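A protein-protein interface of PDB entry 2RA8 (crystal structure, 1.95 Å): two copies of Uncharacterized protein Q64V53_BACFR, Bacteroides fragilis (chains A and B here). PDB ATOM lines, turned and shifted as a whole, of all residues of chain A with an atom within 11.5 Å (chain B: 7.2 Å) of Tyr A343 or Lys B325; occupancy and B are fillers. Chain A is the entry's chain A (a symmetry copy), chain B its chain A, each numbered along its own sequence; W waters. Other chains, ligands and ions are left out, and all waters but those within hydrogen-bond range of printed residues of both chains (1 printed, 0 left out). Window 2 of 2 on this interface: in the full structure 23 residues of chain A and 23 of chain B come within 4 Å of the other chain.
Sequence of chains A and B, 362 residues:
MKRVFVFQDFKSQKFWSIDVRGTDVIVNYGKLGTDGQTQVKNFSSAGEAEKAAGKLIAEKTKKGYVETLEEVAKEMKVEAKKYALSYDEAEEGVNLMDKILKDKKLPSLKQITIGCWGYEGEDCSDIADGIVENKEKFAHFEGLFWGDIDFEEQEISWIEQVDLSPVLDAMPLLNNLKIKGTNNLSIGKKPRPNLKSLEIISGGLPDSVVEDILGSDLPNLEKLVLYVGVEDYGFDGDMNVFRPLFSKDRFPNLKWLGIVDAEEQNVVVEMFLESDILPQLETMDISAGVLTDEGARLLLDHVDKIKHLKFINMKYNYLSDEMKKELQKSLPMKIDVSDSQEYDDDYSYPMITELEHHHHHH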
ATOM      1  N   ASN A 266       4.142  23.564 -17.519  1.00  0.00           N
ATOM      2  CA  ASN A 266       4.065  22.548 -18.564  1.00  0.00           C
ATOM      3  C   ASN A 266       5.413  22.287 -19.178  1.00  0.00           C
ATOM      4  O   ASN A 266       5.709  21.164 -19.594  1.00  0.00           O
ATOM      5  CB  ASN A 266       3.089  22.962 -19.684  1.00  0.00           C
ATOM      6  CG  ASN A 266       1.670  23.211 -19.184  1.00  0.00           C
ATOM      7  OD1 ASN A 266       1.191  22.563 -18.241  1.00  0.00           O
ATOM      8  ND2 ASN A 266       0.982  24.142 -19.831  1.00  0.00           N
ATOM      9  N   GLY A 289       2.309  24.682  -9.447  1.00  0.00           N
ATOM     10  CA  GLY A 289       2.328  25.602 -10.576  1.00  0.00           C
ATOM     11  C   GLY A 289       1.104  25.597 -11.476  1.00  0.00           C
ATOM     12  O   GLY A 289       0.075  24.981 -11.161  1.00  0.00           O
ATOM     13  N   VAL A 290       1.216  26.293 -12.607  1.00  0.00           N
ATOM     14  CA  VAL A 290       0.131  26.365 -13.577  1.00  0.00           C
ATOM     15  C   VAL A 290       0.255  25.224 -14.556  1.00  0.00           C
ATOM     16  O   VAL A 290       0.534  25.416 -15.736  1.00  0.00           O
ATOM     17  CB  VAL A 290       0.151  27.703 -14.340  1.00  0.00           C
ATOM     18  CG1 VAL A 290      -1.043  27.792 -15.272  1.00  0.00           C
ATOM     19  CG2 VAL A 290       0.135  28.851 -13.349  1.00  0.00           C
ATOM     20  N   LEU A 291       0.058  24.018 -14.038  1.00  0.00           N
ATOM     21  CA  LEU A 291       0.125  22.793 -14.816  1.00  0.00           C
ATOM     22  C   LEU A 291      -1.263  22.606 -15.396  1.00  0.00           C
ATOM     23  O   LEU A 291      -2.237  22.433 -14.651  1.00  0.00           O
ATOM     24  CB  LEU A 291       0.457  21.636 -13.885  1.00  0.00           C
ATOM     25  CG  LEU A 291       1.198  20.351 -14.264  1.00  0.00           C
ATOM     26  CD1 LEU A 291       0.395  19.192 -13.704  1.00  0.00           C
ATOM     27  CD2 LEU A 291       1.397  20.211 -15.746  1.00  0.00           C
ATOM     28  N   THR A 292      -1.363  22.662 -16.722  1.00  0.00           N
ATOM     29  CA  THR A 292      -2.647  22.502 -17.403  1.00  0.00           C
ATOM     30  C   THR A 292      -2.742  21.183 -18.117  1.00  0.00           C
ATOM     31  O   THR A 292      -1.785  20.408 -18.147  1.00  0.00           O
ATOM     32  CB  THR A 292      -2.875  23.619 -18.431  1.00  0.00           C
ATOM     33  OG1 THR A 292      -1.824  23.586 -19.406  1.00  0.00           O
ATOM     34  CG2 THR A 292      -2.897  24.972 -17.749  1.00  0.00           C
ATOM     35  N   ASP A 293      -3.903  20.928 -18.713  1.00  0.00           N
ATOM     36  CA  ASP A 293      -4.147  19.681 -19.432  1.00  0.00           C
ATOM     37  C   ASP A 293      -3.165  19.393 -20.538  1.00  0.00           C
ATOM     38  O   ASP A 293      -2.903  18.233 -20.848  1.00  0.00           O
ATOM     39  CB  ASP A 293      -5.565  19.670 -20.012  1.00  0.00           C
ATOM     40  CG  ASP A 293      -6.633  19.511 -18.944  1.00  0.00           C
ATOM     41  OD1 ASP A 293      -6.281  19.243 -17.775  1.00  0.00           O
ATOM     42  OD2 ASP A 293      -7.828  19.647 -19.276  1.00  0.00           O
ATOM     43  N   GLU A 294      -2.626  20.435 -21.161  1.00  0.00           N
ATOM     44  CA  GLU A 294      -1.661  20.213 -22.228  1.00  0.00           C
ATOM     45  C   GLU A 294      -0.362  19.726 -21.643  1.00  0.00           C
ATOM     46  O   GLU A 294       0.462  19.126 -22.335  1.00  0.00           O
ATOM     47  CB  GLU A 294      -1.448  21.489 -23.057  1.00  0.00           C
ATOM     48  CG  GLU A 294      -1.369  22.771 -22.264  1.00  0.00           C
ATOM     49  CD  GLU A 294      -1.355  23.995 -23.164  1.00  0.00           C
ATOM     50  OE1 GLU A 294      -1.374  25.127 -22.634  1.00  0.00           O
ATOM     51  OE2 GLU A 294      -1.324  23.823 -24.401  1.00  0.00           O
ATOM     52  N   GLY A 295      -0.185  19.969 -20.350  1.00  0.00           N
ATOM     53  CA  GLY A 295       1.014  19.511 -19.677  1.00  0.00           C
ATOM     54  C   GLY A 295       0.854  18.038 -19.353  1.00  0.00           C
ATOM     55  O   GLY A 295       1.739  17.226 -19.639  1.00  0.00           O
ATOM     56  N   TYR A 316      -1.766  20.868  -6.481  1.00  0.00           N
ATOM     57  CA  TYR A 316      -1.997  22.271  -6.857  1.00  0.00           C
ATOM     58  C   TYR A 316      -1.732  22.332  -8.340  1.00  0.00           C
ATOM     59  O   TYR A 316      -0.580  22.303  -8.793  1.00  0.00           O
ATOM     60  CB  TYR A 316      -1.091  23.275  -6.120  1.00  0.00           C
ATOM     61  CG  TYR A 316      -1.431  24.721  -6.473  1.00  0.00           C
ATOM     62  CD1 TYR A 316      -0.904  25.321  -7.620  1.00  0.00           C
ATOM     63  CD2 TYR A 316      -2.364  25.448  -5.725  1.00  0.00           C
ATOM     64  CE1 TYR A 316      -1.301  26.597  -8.021  1.00  0.00           C
ATOM     65  CE2 TYR A 316      -2.769  26.734  -6.125  1.00  0.00           C
ATOM     66  CZ  TYR A 316      -2.232  27.292  -7.274  1.00  0.00           C
ATOM     67  OH  TYR A 316      -2.628  28.541  -7.704  1.00  0.00           O
ATOM     68  N   ASN A 317      -2.814  22.409  -9.107  1.00  0.00           N
ATOM     69  CA  ASN A 317      -2.727  22.422 -10.562  1.00  0.00           C
ATOM     70  C   ASN A 317      -3.936  23.078 -11.188  1.00  0.00           C
ATOM     71  O   ASN A 317      -4.805  23.610 -10.498  1.00  0.00           O
ATOM     72  CB  ASN A 317      -2.636  20.981 -11.067  1.00  0.00           C
ATOM     73  CG  ASN A 317      -3.864  20.160 -10.696  1.00  0.00           C
ATOM     74  OD1 ASN A 317      -4.973  20.445 -11.151  1.00  0.00           O
ATOM     75  ND2 ASN A 317      -3.673  19.145  -9.860  1.00  0.00           N
ATOM     76  N   TYR A 318      -3.999  23.029 -12.513  1.00  0.00           N
ATOM     77  CA  TYR A 318      -5.114  23.604 -13.251  1.00  0.00           C
ATOM     78  C   TYR A 318      -5.613  22.588 -14.258  1.00  0.00           C
ATOM     79  O   TYR A 318      -5.906  22.927 -15.400  1.00  0.00           O
ATOM     80  CB  TYR A 318      -4.681  24.898 -13.964  1.00  0.00           C
ATOM     81  CG  TYR A 318      -4.693  26.143 -13.100  1.00  0.00           C
ATOM     82  CD1 TYR A 318      -5.843  26.930 -12.992  1.00  0.00           C
ATOM     83  CD2 TYR A 318      -3.557  26.542 -12.396  1.00  0.00           C
ATOM     84  CE1 TYR A 318      -5.856  28.088 -12.203  1.00  0.00           C
ATOM     85  CE2 TYR A 318      -3.562  27.695 -11.607  1.00  0.00           C
ATOM     86  CZ  TYR A 318      -4.710  28.459 -11.518  1.00  0.00           C
ATOM     87  OH  TYR A 318      -4.704  29.598 -10.752  1.00  0.00           O
ATOM     88  N   LEU A 319      -5.693  21.331 -13.829  1.00  0.00           N
ATOM     89  CA  LEU A 319      -6.177  20.250 -14.679  1.00  0.00           C
ATOM     90  C   LEU A 319      -7.690  20.213 -14.639  1.00  0.00           C
ATOM     91  O   LEU A 319      -8.303  20.626 -13.652  1.00  0.00           O
ATOM     92  CB  LEU A 319      -5.653  18.900 -14.188  1.00  0.00           C
ATOM     93  CG  LEU A 319      -4.137  18.674 -14.145  1.00  0.00           C
ATOM     94  CD1 LEU A 319      -3.863  17.265 -13.650  1.00  0.00           C
ATOM     95  CD2 LEU A 319      -3.533  18.885 -15.529  1.00  0.00           C
ATOM     96  N   SER A 320      -8.303  19.718 -15.709  1.00  0.00           N
ATOM     97  CA  SER A 320      -9.759  19.611 -15.770  1.00  0.00           C
ATOM     98  C   SER A 320     -10.121  18.291 -15.135  1.00  0.00           C
ATOM     99  O   SER A 320      -9.270  17.400 -15.030  1.00  0.00           O
ATOM    100  CB  SER A 320     -10.234  19.633 -17.228  1.00  0.00           C
ATOM    101  OG  SER A 320      -9.757  18.506 -17.942  1.00  0.00           O
ATOM    102  N   ASP A 321     -11.367  18.133 -14.693  1.00  0.00           N
ATOM    103  CA  ASP A 321     -11.727  16.862 -14.084  1.00  0.00           C
ATOM    104  C   ASP A 321     -11.617  15.721 -15.061  1.00  0.00           C
ATOM    105  O   ASP A 321     -11.277  14.603 -14.680  1.00  0.00           O
ATOM    106  CB  ASP A 321     -13.140  16.890 -13.478  1.00  0.00           C
ATOM    107  CG  ASP A 321     -14.108  17.746 -14.262  1.00  0.00           C
ATOM    108  OD1 ASP A 321     -14.026  17.771 -15.509  1.00  0.00           O
ATOM    109  OD2 ASP A 321     -14.971  18.382 -13.619  1.00  0.00           O
ATOM    110  N   GLU A 322     -11.885  15.987 -16.332  1.00  0.00           N
ATOM    111  CA  GLU A 322     -11.802  14.937 -17.338  1.00  0.00           C
ATOM    112  C   GLU A 322     -10.377  14.450 -17.488  1.00  0.00           C
ATOM    113  O   GLU A 322     -10.139  13.247 -17.642  1.00  0.00           O
ATOM    114  CB  GLU A 322     -12.338  15.450 -18.673  1.00  0.00           C
ATOM    115  CG  GLU A 322     -13.722  16.086 -18.545  1.00  0.00           C
ATOM    116  CD  GLU A 322     -14.365  16.400 -19.883  1.00  0.00           C
ATOM    117  OE1 GLU A 322     -13.727  17.091 -20.707  1.00  0.00           O
ATOM    118  OE2 GLU A 322     -15.513  15.959 -20.107  1.00  0.00           O
ATOM    119  N   MET A 323      -9.419  15.375 -17.431  1.00  0.00           N
ATOM    120  CA  MET A 323      -8.003  15.021 -17.547  1.00  0.00           C
ATOM    121  C   MET A 323      -7.537  14.273 -16.318  1.00  0.00           C
ATOM    122  O   MET A 323      -6.745  13.322 -16.411  1.00  0.00           O
ATOM    123  CB  MET A 323      -7.145  16.282 -17.745  1.00  0.00           C
ATOM    124  CG  MET A 323      -5.641  16.021 -17.728  1.00  0.00           C
ATOM    125  SD  MET A 323      -5.052  14.705 -19.036  1.00  0.00           S
ATOM    126  CE  MET A 323      -4.942  15.871 -20.578  1.00  0.00           C
ATOM    127  N   LYS A 324      -8.022  14.689 -15.150  1.00  0.00           N
ATOM    128  CA  LYS A 324      -7.659  14.017 -13.911  1.00  0.00           C
ATOM    129  C   LYS A 324      -8.184  12.598 -13.909  1.00  0.00           C
ATOM    130  O   LYS A 324      -7.518  11.689 -13.412  1.00  0.00           O
ATOM    131  CB  LYS A 324      -8.183  14.798 -12.688  1.00  0.00           C
ATOM    132  CG  LYS A 324      -7.376  16.067 -12.379  1.00  0.00           C
ATOM    133  CD  LYS A 324      -7.882  16.796 -11.131  1.00  0.00           C
ATOM    134  CE  LYS A 324      -9.201  17.506 -11.406  1.00  0.00           C
ATOM    135  NZ  LYS A 324      -9.754  18.172 -10.191  1.00  0.00           N
ATOM    136  N   ASP A 339      -5.984  19.575  -5.021  1.00  0.00           N
ATOM    137  CA  ASP A 339      -5.915  21.029  -5.013  1.00  0.00           C
ATOM    138  C   ASP A 339      -5.966  21.676  -6.367  1.00  0.00           C
ATOM    139  O   ASP A 339      -5.312  22.697  -6.604  1.00  0.00           O
ATOM    140  CB  ASP A 339      -4.666  21.498  -4.263  1.00  0.00           C
ATOM    141  CG  ASP A 339      -4.876  21.544  -2.757  1.00  0.00           C
ATOM    142  OD1 ASP A 339      -5.683  22.380  -2.297  1.00  0.00           O
ATOM    143  OD2 ASP A 339      -4.242  20.746  -2.033  1.00  0.00           O
ATOM    144  N   SER A 340      -6.744  21.092  -7.270  1.00  0.00           N
ATOM    145  CA  SER A 340      -6.900  21.658  -8.600  1.00  0.00           C
ATOM    146  C   SER A 340      -7.579  22.991  -8.442  1.00  0.00           C
ATOM    147  O   SER A 340      -8.470  23.147  -7.609  1.00  0.00           O
ATOM    148  CB  SER A 340      -7.773  20.754  -9.486  1.00  0.00           C
ATOM    149  OG  SER A 340      -7.139  19.515  -9.750  1.00  0.00           O
ATOM    150  N   GLN A 341      -7.156  23.967  -9.233  1.00  0.00           N
ATOM    151  CA  GLN A 341      -7.751  25.290  -9.177  1.00  0.00           C
ATOM    152  C   GLN A 341      -8.743  25.405 -10.306  1.00  0.00           C
ATOM    153  O   GLN A 341      -8.844  24.501 -11.137  1.00  0.00           O
ATOM    154  CB  GLN A 341      -6.671  26.362  -9.319  1.00  0.00           C
ATOM    155  CG  GLN A 341      -5.527  26.237  -8.310  1.00  0.00           C
ATOM    156  CD  GLN A 341      -5.997  26.309  -6.863  1.00  0.00           C
ATOM    157  OE1 GLN A 341      -6.075  25.297  -6.166  1.00  0.00           O
ATOM    158  NE2 GLN A 341      -6.320  27.513  -6.410  1.00  0.00           N
ATOM    159  N   GLU A 342      -9.487  26.507 -10.342  1.00  0.00           N
ATOM    160  CA  GLU A 342     -10.476  26.703 -11.399  1.00  0.00           C
ATOM    161  C   GLU A 342      -9.850  27.378 -12.592  1.00  0.00           C
ATOM    162  O   GLU A 342      -9.443  28.537 -12.523  1.00  0.00           O
ATOM    163  CB  GLU A 342     -11.657  27.539 -10.885  1.00  0.00           C
ATOM    164  CG  GLU A 342     -12.869  27.522 -11.811  1.00  0.00           C
ATOM    165  CD  GLU A 342     -14.118  28.111 -11.175  1.00  0.00           C
ATOM    166  OE1 GLU A 342     -15.194  28.040 -11.807  1.00  0.00           O
ATOM    167  OE2 GLU A 342     -14.028  28.644 -10.048  1.00  0.00           O
ATOM    168  N   TYR A 343      -9.760  26.638 -13.693  1.00  0.00           N
ATOM    169  CA  TYR A 343      -9.171  27.149 -14.926  1.00  0.00           C
ATOM    170  C   TYR A 343     -10.113  28.081 -15.646  1.00  0.00           C
ATOM    171  O   TYR A 343      -9.682  29.029 -16.307  1.00  0.00           O
ATOM    172  CB  TYR A 343      -8.786  25.985 -15.836  1.00  0.00           C
ATOM    173  N   PRO A 350      -6.741  35.271 -14.052  1.00  0.00           N
ATOM    174  CA  PRO A 350      -5.405  34.811 -14.453  1.00  0.00           C
ATOM    175  C   PRO A 350      -4.952  33.669 -13.594  1.00  0.00           C
ATOM    176  O   PRO A 350      -5.133  33.690 -12.379  1.00  0.00           O
ATOM    177  CB  PRO A 350      -4.532  36.048 -14.251  1.00  0.00           C
ATOM    178  CG  PRO A 350      -5.490  37.176 -14.489  1.00  0.00           C
ATOM    179  CD  PRO A 350      -6.728  36.713 -13.752  1.00  0.00           C
ATOM    180  N   MET A 351      -4.360  32.656 -14.214  1.00  0.00           N
ATOM    181  CA  MET A 351      -3.883  31.505 -13.468  1.00  0.00           C
ATOM    182  C   MET A 351      -2.558  31.832 -12.836  1.00  0.00           C
ATOM    183  O   MET A 351      -1.638  32.313 -13.505  1.00  0.00           O
ATOM    184  CB  MET A 351      -3.749  30.302 -14.397  1.00  0.00           C
ATOM    185  CG  MET A 351      -5.062  29.906 -15.056  1.00  0.00           C
ATOM    186  SD  MET A 351      -4.893  28.364 -16.209  1.00  0.00           S
ATOM    187  CE  MET A 351      -4.114  29.254 -17.749  1.00  0.00           C
ATOM    188  N   ILE A 352      -2.458  31.574 -11.536  1.00  0.00           N
ATOM    189  CA  ILE A 352      -1.241  31.868 -10.789  1.00  0.00           C
ATOM    190  C   ILE A 352      -0.648  30.666 -10.101  1.00  0.00           C
ATOM    191  O   ILE A 352      -1.296  29.621  -9.977  1.00  0.00           O
ATOM    192  CB  ILE A 352      -1.514  32.950  -9.730  1.00  0.00           C
ATOM    193  CG1 ILE A 352      -2.627  32.485  -8.791  1.00  0.00           C
ATOM    194  CG2 ILE A 352      -1.908  34.249 -10.411  1.00  0.00           C
ATOM    195  CD1 ILE A 352      -2.941  33.462  -7.665  1.00  0.00           C
ATOM    196  N   SER B 320     -18.644  19.700 -10.487  1.00  0.00           N
ATOM    197  CA  SER B 320     -17.810  19.443 -11.659  1.00  0.00           C
ATOM    198  C   SER B 320     -17.402  20.789 -12.202  1.00  0.00           C
ATOM    199  O   SER B 320     -18.050  21.799 -11.904  1.00  0.00           O
ATOM    200  CB  SER B 320     -18.606  18.674 -12.721  1.00  0.00           C
ATOM    201  OG  SER B 320     -19.690  19.445 -13.210  1.00  0.00           O
ATOM    202  N   ASP B 321     -16.332  20.844 -12.992  1.00  0.00           N
ATOM    203  CA  ASP B 321     -15.933  22.138 -13.525  1.00  0.00           C
ATOM    204  C   ASP B 321     -16.990  22.723 -14.425  1.00  0.00           C
ATOM    205  O   ASP B 321     -17.163  23.939 -14.475  1.00  0.00           O
ATOM    206  CB  ASP B 321     -14.594  22.066 -14.277  1.00  0.00           C
ATOM    207  CG  ASP B 321     -14.392  20.761 -15.012  1.00  0.00           C
ATOM    208  OD1 ASP B 321     -15.375  20.207 -15.550  1.00  0.00           O
ATOM    209  OD2 ASP B 321     -13.231  20.300 -15.065  1.00  0.00           O
ATOM    210  N   GLU B 322     -17.720  21.872 -15.131  1.00  0.00           N
ATOM    211  CA  GLU B 322     -18.761  22.358 -16.026  1.00  0.00           C
ATOM    212  C   GLU B 322     -19.867  23.034 -15.242  1.00  0.00           C
ATOM    213  O   GLU B 322     -20.398  24.064 -15.670  1.00  0.00           O
ATOM    214  CB  GLU B 322     -19.317  21.204 -16.857  1.00  0.00           C
ATOM    215  CG  GLU B 322     -18.220  20.400 -17.554  1.00  0.00           C
ATOM    216  CD  GLU B 322     -18.757  19.393 -18.554  1.00  0.00           C
ATOM    217  OE1 GLU B 322     -19.619  18.571 -18.174  1.00  0.00           O
ATOM    218  OE2 GLU B 322     -18.311  19.422 -19.722  1.00  0.00           O
ATOM    219  N   MET B 323     -20.213  22.467 -14.087  1.00  0.00           N
ATOM    220  CA  MET B 323     -21.258  23.039 -13.235  1.00  0.00           C
ATOM    221  C   MET B 323     -20.789  24.335 -12.613  1.00  0.00           C
ATOM    222  O   MET B 323     -21.563  25.297 -12.483  1.00  0.00           O
ATOM    223  CB  MET B 323     -21.659  22.047 -12.131  1.00  0.00           C
ATOM    224  CG  MET B 323     -22.638  22.615 -11.107  1.00  0.00           C
ATOM    225  SD  MET B 323     -24.280  23.313 -11.886  1.00  0.00           S
ATOM    226  CE  MET B 323     -25.248  21.644 -12.045  1.00  0.00           C
ATOM    227  N   LYS B 324     -19.518  24.381 -12.221  1.00  0.00           N
ATOM    228  CA  LYS B 324     -18.961  25.593 -11.638  1.00  0.00           C
ATOM    229  C   LYS B 324     -18.950  26.711 -12.658  1.00  0.00           C
ATOM    230  O   LYS B 324     -19.193  27.869 -12.314  1.00  0.00           O
ATOM    231  CB  LYS B 324     -17.544  25.337 -11.087  1.00  0.00           C
ATOM    232  CG  LYS B 324     -17.530  24.550  -9.769  1.00  0.00           C
ATOM    233  CD  LYS B 324     -16.115  24.355  -9.216  1.00  0.00           C
ATOM    234  CE  LYS B 324     -15.345  23.322 -10.029  1.00  0.00           C
ATOM    235  NZ  LYS B 324     -13.940  23.156  -9.555  1.00  0.00           N
ATOM    236  N   LYS B 325     -18.695  26.382 -13.924  1.00  0.00           N
ATOM    237  CA  LYS B 325     -18.701  27.399 -14.977  1.00  0.00           C
ATOM    238  C   LYS B 325     -20.105  27.942 -15.110  1.00  0.00           C
ATOM    239  O   LYS B 325     -20.311  29.152 -15.182  1.00  0.00           O
ATOM    240  CB  LYS B 325     -18.296  26.805 -16.330  1.00  0.00           C
ATOM    241  CG  LYS B 325     -16.919  26.170 -16.389  1.00  0.00           C
ATOM    242  CD  LYS B 325     -15.796  27.194 -16.361  1.00  0.00           C
ATOM    243  CE  LYS B 325     -14.442  26.500 -16.502  1.00  0.00           C
ATOM    244  NZ  LYS B 325     -13.304  27.453 -16.594  1.00  0.00           N
ATOM    245  N   GLU B 326     -21.080  27.035 -15.143  1.00  0.00           N
ATOM    246  CA  GLU B 326     -22.487  27.405 -15.281  1.00  0.00           C
ATOM    247  C   GLU B 326     -22.921  28.275 -14.141  1.00  0.00           C
ATOM    248  O   GLU B 326     -23.558  29.309 -14.341  1.00  0.00           O
ATOM    249  CB  GLU B 326     -23.373  26.162 -15.313  1.00  0.00           C
ATOM    250  CG  GLU B 326     -24.684  26.372 -16.062  1.00  0.00           C
ATOM    251  CD  GLU B 326     -25.570  25.139 -16.062  1.00  0.00           C
ATOM    252  OE1 GLU B 326     -25.028  24.017 -16.148  1.00  0.00           O
ATOM    253  OE2 GLU B 326     -26.808  25.290 -15.991  1.00  0.00           O
ATOM    254  N   LEU B 327     -22.579  27.856 -12.929  1.00  0.00           N
ATOM    255  CA  LEU B 327     -22.926  28.615 -11.733  1.00  0.00           C
ATOM    256  C   LEU B 327     -22.314  29.983 -11.790  1.00  0.00           C
ATOM    257  O   LEU B 327     -22.958  30.981 -11.463  1.00  0.00           O
ATOM    258  CB  LEU B 327     -22.421  27.895 -10.481  1.00  0.00           C
ATOM    259  CG  LEU B 327     -23.152  26.606 -10.121  1.00  0.00           C
ATOM    260  CD1 LEU B 327     -22.340  25.830  -9.106  1.00  0.00           C
ATOM    261  CD2 LEU B 327     -24.539  26.940  -9.584  1.00  0.00           C
ATOM    262  N   GLN B 328     -21.056  30.036 -12.216  1.00  0.00           N
ATOM    263  CA  GLN B 328     -20.324  31.292 -12.321  1.00  0.00           C
ATOM    264  C   GLN B 328     -21.035  32.269 -13.237  1.00  0.00           C
ATOM    265  O   GLN B 328     -21.254  33.429 -12.881  1.00  0.00           O
ATOM    266  CB  GLN B 328     -18.918  31.028 -12.874  1.00  0.00           C
ATOM    267  CG  GLN B 328     -17.765  31.644 -12.083  1.00  0.00           C
ATOM    268  CD  GLN B 328     -17.363  30.812 -10.880  1.00  0.00           C
ATOM    269  OE1 GLN B 328     -16.368  31.101 -10.216  1.00  0.00           O
ATOM    270  NE2 GLN B 328     -18.136  29.773 -10.592  1.00  0.00           N
ATOM    271  N   LYS B 329     -21.410  31.792 -14.422  1.00  0.00           N
ATOM    272  CA  LYS B 329     -22.068  32.629 -15.422  1.00  0.00           C
ATOM    273  C   LYS B 329     -23.544  32.875 -15.214  1.00  0.00           C
ATOM    274  O   LYS B 329     -24.048  33.938 -15.579  1.00  0.00           O
ATOM    275  CB  LYS B 329     -21.865  32.031 -16.817  1.00  0.00           C
ATOM    276  CG  LYS B 329     -22.168  32.994 -17.954  1.00  0.00           C
ATOM    277  CD  LYS B 329     -22.059  32.310 -19.309  1.00  0.00           C
ATOM    278  CE  LYS B 329     -22.062  33.329 -20.443  1.00  0.00           C
ATOM    279  NZ  LYS B 329     -23.253  34.221 -20.399  1.00  0.00           N
ATOM    280  N   SER B 330     -24.248  31.905 -14.636  1.00  0.00           N
ATOM    281  CA  SER B 330     -25.685  32.039 -14.414  1.00  0.00           C
ATOM    282  C   SER B 330     -26.095  32.723 -13.120  1.00  0.00           C
ATOM    283  O   SER B 330     -27.220  33.207 -13.011  1.00  0.00           O
ATOM    284  CB  SER B 330     -26.356  30.664 -14.490  1.00  0.00           C
ATOM    285  OG  SER B 330     -26.177  30.080 -15.770  1.00  0.00           O
ATOM    286  N   LEU B 331     -25.207  32.770 -12.131  1.00  0.00           N
ATOM    287  CA  LEU B 331     -25.546  33.431 -10.869  1.00  0.00           C
ATOM    288  C   LEU B 331     -24.971  34.826 -10.829  1.00  0.00           C
ATOM    289  O   LEU B 331     -23.780  35.024 -11.053  1.00  0.00           O
ATOM    290  CB  LEU B 331     -25.049  32.600  -9.675  1.00  0.00           C
ATOM    291  CG  LEU B 331     -25.744  31.234  -9.519  1.00  0.00           C
ATOM    292  CD1 LEU B 331     -25.269  30.542  -8.254  1.00  0.00           C
ATOM    293  CD2 LEU B 331     -27.254  31.431  -9.465  1.00  0.00           C
ATOM    294  N   VAL B 337     -16.952  28.769  -4.944  1.00  0.00           N
ATOM    295  CA  VAL B 337     -17.030  27.361  -5.301  1.00  0.00           C
ATOM    296  C   VAL B 337     -15.668  26.721  -5.219  1.00  0.00           C
ATOM    297  O   VAL B 337     -15.450  25.639  -5.756  1.00  0.00           O
ATOM    298  CB  VAL B 337     -17.616  27.183  -6.722  1.00  0.00           C
ATOM    299  CG1 VAL B 337     -19.116  27.402  -6.690  1.00  0.00           C
ATOM    300  CG2 VAL B 337     -16.978  28.182  -7.679  1.00  0.00           C
HETATM  301  O   HOH W   1     -14.893  25.202 -13.702  1.00  0.00           O
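Ser A320 touches Asp B321, and with the chains exchanged Asp A321 touches Ser B320. Asp A321 touches its own counterpart, Asp B321. Of the 7 pairs that touch across the chains among the printed residues, 3 have their exchanged pair printed and touching as well.
Among the printed residues, pairs that only touch across the chains: Ser A320 with Asp B321 (3.6 Å), Asp A321 with Ser B320 (3.6 Å), Glu A342 with Lys B324 (3.7 Å), Glu A342 with Val B337 (3.8 Å) and Tyr A343 with Lys B325 (3.4 Å).
The backbone NH of Asp B321 sits close to the side-chain carboxylate of Asp A321, at 2.9 Å. The side-chain amide oxygen of Gln B328 sits close to the side-chain carboxylate of Glu A342, 3.4 Å away.
The side-chain hydroxyl (OG) of Ser A320 sits at hydrogen-bond distance from the backbone NH (N) of Met A323, at 3.2 Å. The side-chain hydroxyl (OG) of Ser B320 sits at hydrogen-bond distance from the backbone NH (N) of Met B323 (3.2 Å). OD2 of Asp A293 lies within hydrogen-bond range of OG of Ser A320 (2.6 Å). The backbone carbonyl oxygen (O) of Lys B324 lies within hydrogen-bond range of the side-chain amide nitrogen (NE2) of Gln B328.
Along chain B the printed residues that touch a printed residue of chain A span positions 320 to 337. Printed residues of chain A that touch a printed residue of chain B: Ser A320, Asp A321, Glu A342 and Tyr A343. Among the printed residues, no Asp or Glu carboxylate lies within 4 Å of a Lys or Arg side-chain nitrogen of the other chain.
Of the printed residues of chain B, Tyr A343 touches Lys B325 (3.4 Å). Of chain A, only Tyr A343 comes within 4 Å of Lys B325. Asp B321 touches just these residues of chain A: Ser A320 and Asp A321. Of chain A, only Glu A342 (3.7 Å) comes within 4 Å of Lys B324. No residue of chain A comes within 4 Å of Glu B326. No residue of chain A comes within 4 Å of Leu B327. Of chain A, only Glu A342 (3.4 Å) comes within 4 Å of Gln B328. Of the printed residues of chain A, Val B337 touches Glu A342 (3.8 Å). Of the printed residues of chain A, Ser B320 touches Asp A321 (3.6 Å). Printed residues of chain B within 4 Å of Ser A320: Asp B321. Printed residues of chain B within 4 Å of Glu A342: Lys B324, Gln B328 and Val B337. Of the printed residues of chain B, Asp A321 touches Ser B320 (3.6 Å) and Asp B321 (2.7 Å). Gln A341 touches none of the printed residues of chain B. The nearest residue of chain B that does not touch Tyr A343 is Asp B321 (6.7 Å). The nearest residue of chain A that does not touch Lys B325 is Glu A342 (4.4 Å).
Water W1 lies within hydrogen-bond range of the backbone carbonyl oxygen of Asp B321 (2.7 Å) and the side-chain carboxylate of Glu A342 (3.4 Å).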
